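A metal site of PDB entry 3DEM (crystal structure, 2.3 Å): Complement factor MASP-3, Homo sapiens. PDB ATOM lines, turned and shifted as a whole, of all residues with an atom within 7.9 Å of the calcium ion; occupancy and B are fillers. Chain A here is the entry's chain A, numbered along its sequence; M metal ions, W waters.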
ATOM      1  N   TYR A 187     -14.795 -10.565  13.637  1.00  0.00           N
ATOM      2  CA  TYR A 187     -15.832  -9.855  14.377  1.00  0.00           C
ATOM      3  C   TYR A 187     -17.174 -10.589  14.347  1.00  0.00           C
ATOM      4  O   TYR A 187     -17.488 -11.284  13.378  1.00  0.00           O
ATOM      5  CB  TYR A 187     -15.986  -8.404  13.885  1.00  0.00           C
ATOM      6  CG  TYR A 187     -16.208  -8.233  12.393  1.00  0.00           C
ATOM      7  CD1 TYR A 187     -17.459  -8.421  11.825  1.00  0.00           C
ATOM      8  CD2 TYR A 187     -15.163  -7.824  11.572  1.00  0.00           C
ATOM      9  CE1 TYR A 187     -17.660  -8.240  10.459  1.00  0.00           C
ATOM     10  CE2 TYR A 187     -15.360  -7.626  10.217  1.00  0.00           C
ATOM     11  CZ  TYR A 187     -16.604  -7.835   9.660  1.00  0.00           C
ATOM     12  OH  TYR A 187     -16.783  -7.649   8.298  1.00  0.00           O
ATOM     13  N   PRO A 188     -17.955 -10.455  15.432  1.00  0.00           N
ATOM     14  CA  PRO A 188     -19.263 -11.116  15.557  1.00  0.00           C
ATOM     15  C   PRO A 188     -20.229 -10.712  14.442  1.00  0.00           C
ATOM     16  O   PRO A 188     -20.306  -9.549  14.066  1.00  0.00           O
ATOM     17  CB  PRO A 188     -19.781 -10.607  16.905  1.00  0.00           C
ATOM     18  CG  PRO A 188     -18.563 -10.231  17.663  1.00  0.00           C
ATOM     19  CD  PRO A 188     -17.618  -9.680  16.643  1.00  0.00           C
ATOM     20  N   LYS A 189     -20.962 -11.702  13.931  1.00  0.00           N
ATOM     21  CA  LYS A 189     -21.973 -11.471  12.929  1.00  0.00           C
ATOM     22  C   LYS A 189     -23.187 -10.792  13.559  1.00  0.00           C
ATOM     23  O   LYS A 189     -23.334 -10.763  14.783  1.00  0.00           O
ATOM     24  CB  LYS A 189     -22.410 -12.800  12.309  1.00  0.00           C
ATOM     25  CG  LYS A 189     -21.287 -13.554  11.604  1.00  0.00           C
ATOM     26  CD  LYS A 189     -21.761 -14.911  11.095  1.00  0.00           C
ATOM     27  CE  LYS A 189     -20.619 -15.700  10.475  1.00  0.00           C
ATOM     28  NZ  LYS A 189     -19.549 -16.047  11.464  1.00  0.00           N
ATOM     29  N   SER A 190     -24.043 -10.230  12.704  1.00  0.00           N
ATOM     30  CA  SER A 190     -25.361  -9.747  13.110  1.00  0.00           C
ATOM     31  C   SER A 190     -25.337  -8.763  14.262  1.00  0.00           C
ATOM     32  O   SER A 190     -26.241  -8.758  15.105  1.00  0.00           O
ATOM     33  CB  SER A 190     -26.269 -10.931  13.464  1.00  0.00           C
ATOM     34  OG  SER A 190     -26.382 -11.806  12.365  1.00  0.00           O
ATOM     35  N   ILE A 215     -13.022  -5.523   6.380  1.00  0.00           N
ATOM     36  CA  ILE A 215     -14.469  -5.499   6.473  1.00  0.00           C
ATOM     37  C   ILE A 215     -15.024  -6.033   5.157  1.00  0.00           C
ATOM     38  O   ILE A 215     -14.643  -5.583   4.084  1.00  0.00           O
ATOM     39  CB  ILE A 215     -15.000  -4.067   6.724  1.00  0.00           C
ATOM     40  CG1 ILE A 215     -14.338  -3.479   7.974  1.00  0.00           C
ATOM     41  CG2 ILE A 215     -16.518  -4.074   6.891  1.00  0.00           C
ATOM     42  CD1 ILE A 215     -14.901  -2.132   8.406  1.00  0.00           C
ATOM     43  N   GLU A 216     -15.906  -7.030   5.252  1.00  0.00           N
ATOM     44  CA  GLU A 216     -16.486  -7.641   4.064  1.00  0.00           C
ATOM     45  C   GLU A 216     -17.013  -6.578   3.105  1.00  0.00           C
ATOM     46  O   GLU A 216     -17.705  -5.640   3.520  1.00  0.00           O
ATOM     47  CB  GLU A 216     -17.631  -8.583   4.468  1.00  0.00           C
ATOM     48  CG  GLU A 216     -18.066  -9.548   3.380  1.00  0.00           C
ATOM     49  CD  GLU A 216     -19.313 -10.317   3.760  1.00  0.00           C
ATOM     50  OE1 GLU A 216     -19.823 -10.110   4.879  1.00  0.00           O
ATOM     51  OE2 GLU A 216     -19.790 -11.127   2.935  1.00  0.00           O
ATOM     52  N   ASP A 217     -16.697  -6.722   1.828  1.00  0.00           N
ATOM     53  CA  ASP A 217     -17.202  -5.799   0.815  1.00  0.00           C
ATOM     54  C   ASP A 217     -17.676  -6.524  -0.442  1.00  0.00           C
ATOM     55  O   ASP A 217     -17.665  -7.752  -0.502  1.00  0.00           O
ATOM     56  CB  ASP A 217     -16.161  -4.729   0.477  1.00  0.00           C
ATOM     57  CG  ASP A 217     -14.953  -5.274  -0.282  1.00  0.00           C
ATOM     58  OD1 ASP A 217     -14.851  -6.510  -0.474  1.00  0.00           O
ATOM     59  OD2 ASP A 217     -14.100  -4.465  -0.712  1.00  0.00           O
ATOM     60  N   TYR A 225     -22.912  -5.273   2.799  1.00  0.00           N
ATOM     61  CA  TYR A 225     -22.928  -6.273   3.857  1.00  0.00           C
ATOM     62  C   TYR A 225     -22.596  -5.703   5.235  1.00  0.00           C
ATOM     63  O   TYR A 225     -23.471  -5.601   6.105  1.00  0.00           O
ATOM     64  CB  TYR A 225     -21.952  -7.417   3.525  1.00  0.00           C
ATOM     65  CG  TYR A 225     -22.149  -8.038   2.157  1.00  0.00           C
ATOM     66  CD1 TYR A 225     -23.399  -8.510   1.764  1.00  0.00           C
ATOM     67  CD2 TYR A 225     -21.094  -8.146   1.268  1.00  0.00           C
ATOM     68  CE1 TYR A 225     -23.580  -9.086   0.509  1.00  0.00           C
ATOM     69  CE2 TYR A 225     -21.263  -8.715   0.018  1.00  0.00           C
ATOM     70  CZ  TYR A 225     -22.511  -9.184  -0.362  1.00  0.00           C
ATOM     71  OH  TYR A 225     -22.678  -9.746  -1.607  1.00  0.00           O
ATOM     72  N   ASP A 226     -21.325  -5.361   5.427  1.00  0.00           N
ATOM     73  CA  ASP A 226     -20.837  -4.779   6.675  1.00  0.00           C
ATOM     74  C   ASP A 226     -20.283  -3.387   6.391  1.00  0.00           C
ATOM     75  O   ASP A 226     -19.922  -3.073   5.253  1.00  0.00           O
ATOM     76  CB  ASP A 226     -19.730  -5.647   7.274  1.00  0.00           C
ATOM     77  CG  ASP A 226     -20.100  -7.117   7.351  1.00  0.00           C
ATOM     78  OD1 ASP A 226     -21.310  -7.454   7.427  1.00  0.00           O
ATOM     79  OD2 ASP A 226     -19.175  -7.951   7.346  1.00  0.00           O
ATOM     80  N   TYR A 227     -20.192  -2.546   7.420  1.00  0.00           N
ATOM     81  CA  TYR A 227     -19.700  -1.191   7.215  1.00  0.00           C
ATOM     82  C   TYR A 227     -19.509  -0.400   8.490  1.00  0.00           C
ATOM     83  O   TYR A 227     -20.079  -0.705   9.540  1.00  0.00           O
ATOM     84  CB  TYR A 227     -20.635  -0.413   6.281  1.00  0.00           C
ATOM     85  CG  TYR A 227     -22.071  -0.377   6.763  1.00  0.00           C
ATOM     86  CD1 TYR A 227     -22.490   0.564   7.692  1.00  0.00           C
ATOM     87  CD2 TYR A 227     -23.012  -1.295   6.289  1.00  0.00           C
ATOM     88  CE1 TYR A 227     -23.797   0.598   8.130  1.00  0.00           C
ATOM     89  CE2 TYR A 227     -24.329  -1.259   6.729  1.00  0.00           C
ATOM     90  CZ  TYR A 227     -24.715  -0.309   7.652  1.00  0.00           C
ATOM     91  OH  TYR A 227     -26.019  -0.259   8.101  1.00  0.00           O
ATOM     92  N   PHE A 260     -20.701   0.538  13.669  1.00  0.00           N
ATOM     93  CA  PHE A 260     -20.206  -0.625  12.960  1.00  0.00           C
ATOM     94  C   PHE A 260     -21.309  -1.669  12.813  1.00  0.00           C
ATOM     95  O   PHE A 260     -21.812  -2.191  13.799  1.00  0.00           O
ATOM     96  CB  PHE A 260     -18.990  -1.228  13.673  1.00  0.00           C
ATOM     97  CG  PHE A 260     -18.421  -2.443  12.981  1.00  0.00           C
ATOM     98  CD1 PHE A 260     -18.185  -2.433  11.608  1.00  0.00           C
ATOM     99  CD2 PHE A 260     -18.110  -3.587  13.712  1.00  0.00           C
ATOM    100  CE1 PHE A 260     -17.666  -3.553  10.974  1.00  0.00           C
ATOM    101  CE2 PHE A 260     -17.581  -4.709  13.077  1.00  0.00           C
ATOM    102  CZ  PHE A 260     -17.365  -4.695  11.706  1.00  0.00           C
ATOM    103  N   HIS A 261     -21.679  -1.953  11.570  1.00  0.00           N
ATOM    104  CA  HIS A 261     -22.737  -2.918  11.286  1.00  0.00           C
ATOM    105  C   HIS A 261     -22.138  -4.170  10.678  1.00  0.00           C
ATOM    106  O   HIS A 261     -21.314  -4.094   9.777  1.00  0.00           O
ATOM    107  CB  HIS A 261     -23.755  -2.303  10.316  1.00  0.00           C
ATOM    108  CG  HIS A 261     -24.892  -3.221   9.951  1.00  0.00           C
ATOM    109  ND1 HIS A 261     -24.855  -4.068   8.865  1.00  0.00           N
ATOM    110  CD2 HIS A 261     -26.098  -3.409  10.526  1.00  0.00           C
ATOM    111  CE1 HIS A 261     -25.986  -4.743   8.798  1.00  0.00           C
ATOM    112  NE2 HIS A 261     -26.760  -4.367   9.789  1.00  0.00           N
ATOM    113  N   SER A 262     -22.552  -5.338  11.184  1.00  0.00           N
ATOM    114  CA  SER A 262     -22.141  -6.609  10.579  1.00  0.00           C
ATOM    115  C   SER A 262     -23.357  -7.481  10.265  1.00  0.00           C
ATOM    116  O   SER A 262     -24.282  -7.568  11.070  1.00  0.00           O
ATOM    117  CB  SER A 262     -21.131  -7.346  11.459  1.00  0.00           C
ATOM    118  OG  SER A 262     -21.723  -7.827  12.657  1.00  0.00           O
ATOM    119  N   ASP A 263     -23.340  -8.128   9.103  1.00  0.00           N
ATOM    120  CA  ASP A 263     -24.456  -8.977   8.700  1.00  0.00           C
ATOM    121  C   ASP A 263     -24.292 -10.424   9.184  1.00  0.00           C
ATOM    122  O   ASP A 263     -23.429 -10.723  10.005  1.00  0.00           O
ATOM    123  CB  ASP A 263     -24.700  -8.910   7.188  1.00  0.00           C
ATOM    124  CG  ASP A 263     -23.620  -9.635   6.381  1.00  0.00           C
ATOM    125  OD1 ASP A 263     -22.678 -10.187   6.984  1.00  0.00           O
ATOM    126  OD2 ASP A 263     -23.725  -9.646   5.145  1.00  0.00           O
ATOM    127  N   ASN A 264     -25.140 -11.323   8.667  1.00  0.00           N
ATOM    128  CA  ASN A 264     -25.224 -12.687   9.168  1.00  0.00           C
ATOM    129  C   ASN A 264     -24.208 -13.675   8.582  1.00  0.00           C
ATOM    130  O   ASN A 264     -24.362 -14.887   8.726  1.00  0.00           O
ATOM    131  CB  ASN A 264     -26.653 -13.220   8.990  1.00  0.00           C
ATOM    132  CG  ASN A 264     -27.014 -13.480   7.537  1.00  0.00           C
ATOM    133  OD1 ASN A 264     -26.200 -13.292   6.636  1.00  0.00           O
ATOM    134  ND2 ASN A 264     -28.244 -13.918   7.309  1.00  0.00           N
ATOM    135  N   SER A 265     -23.159 -13.152   7.941  1.00  0.00           N
ATOM    136  CA  SER A 265     -22.243 -14.012   7.194  1.00  0.00           C
ATOM    137  C   SER A 265     -20.808 -13.460   7.135  1.00  0.00           C
ATOM    138  O   SER A 265     -20.605 -12.259   7.140  1.00  0.00           O
ATOM    139  CB  SER A 265     -22.796 -14.224   5.775  1.00  0.00           C
ATOM    140  OG  SER A 265     -21.910 -15.012   5.001  1.00  0.00           O
ATOM    141  N   GLY A 266     -19.826 -14.362   7.101  1.00  0.00           N
ATOM    142  CA  GLY A 266     -18.420 -13.971   6.927  1.00  0.00           C
ATOM    143  C   GLY A 266     -17.529 -14.116   8.156  1.00  0.00           C
ATOM    144  O   GLY A 266     -18.012 -14.258   9.279  1.00  0.00           O
ATOM    145  N   GLU A 267     -16.212 -14.079   7.941  1.00  0.00           N
ATOM    146  CA  GLU A 267     -15.250 -14.224   9.032  1.00  0.00           C
ATOM    147  C   GLU A 267     -14.171 -13.142   9.035  1.00  0.00           C
ATOM    148  O   GLU A 267     -13.069 -13.345   9.548  1.00  0.00           O
ATOM    149  CB  GLU A 267     -14.584 -15.611   8.981  1.00  0.00           C
ATOM    150  CG  GLU A 267     -15.551 -16.788   8.934  1.00  0.00           C
ATOM    151  CD  GLU A 267     -16.362 -16.943  10.213  1.00  0.00           C
ATOM    152  OE1 GLU A 267     -15.923 -16.438  11.279  1.00  0.00           O
ATOM    153  OE2 GLU A 267     -17.450 -17.558  10.151  1.00  0.00           O
ATOM    154  N   ASN A 268     -14.485 -11.979   8.482  1.00  0.00           N
ATOM    155  CA  ASN A 268     -13.523 -10.884   8.393  1.00  0.00           C
ATOM    156  C   ASN A 268     -12.984 -10.397   9.750  1.00  0.00           C
ATOM    157  O   ASN A 268     -13.663 -10.455  10.776  1.00  0.00           O
ATOM    158  CB  ASN A 268     -14.115  -9.735   7.569  1.00  0.00           C
ATOM    159  CG  ASN A 268     -14.631 -10.209   6.222  1.00  0.00           C
ATOM    160  OD1 ASN A 268     -13.925 -10.117   5.208  1.00  0.00           O
ATOM    161  ND2 ASN A 268     -15.835 -10.757   6.210  1.00  0.00           N
HETATM  162 CA    CA M   1     -20.270 -10.001   7.079  1.00  0.00          CA
HETATM  163  O   HOH W   1     -18.025 -10.648   7.620  1.00  0.00           O
HETATM  164  O   HOH W   2     -20.640 -10.198   9.443  1.00  0.00           O
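Of the 19 residues printed, 4 come within 4 Å of the calcium ion.
The nearest printed residue that does not touch the calcium ion is Tyr 187 (4.4 Å).
The side-chain carboxylate (OE1) of Glu 216 is bound to the calcium ion, at 2.2 Å.
The calcium ion is bound by O of Ser 265 (2.3 Å).
OD2 of Asp 226 is bound to the calcium ion.
Water W1 binds the calcium ion (2.4 Å).
The calcium ion is bound by water W2 (2.4 Å).
The side-chain carboxylate (OD1) of Asp 263 binds the calcium ion, 2.4 Å away.
OD1 of Asp 226 is bound to the calcium ion (2.8 Å).
The calcium ion has seven donor atoms within binding distance.
The backbone NH (N) of Glu 216 is in hydrogen-bond range of the side-chain hydroxyl (OH) of Tyr 187, at 3.2 Å.
The side-chain carboxylate (OD2) of Asp 226 lies close to the side-chain hydroxyl (OH) of Tyr 187 (2.6 Å).
O of Asp 263 sits at hydrogen-bond distance from N of Ser 190 (2.8 Å).
Water W1 lies within hydrogen-bond range of ND2 of Asn 268 (2.6 Å) and OH of Tyr 187 (3.3 Å).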
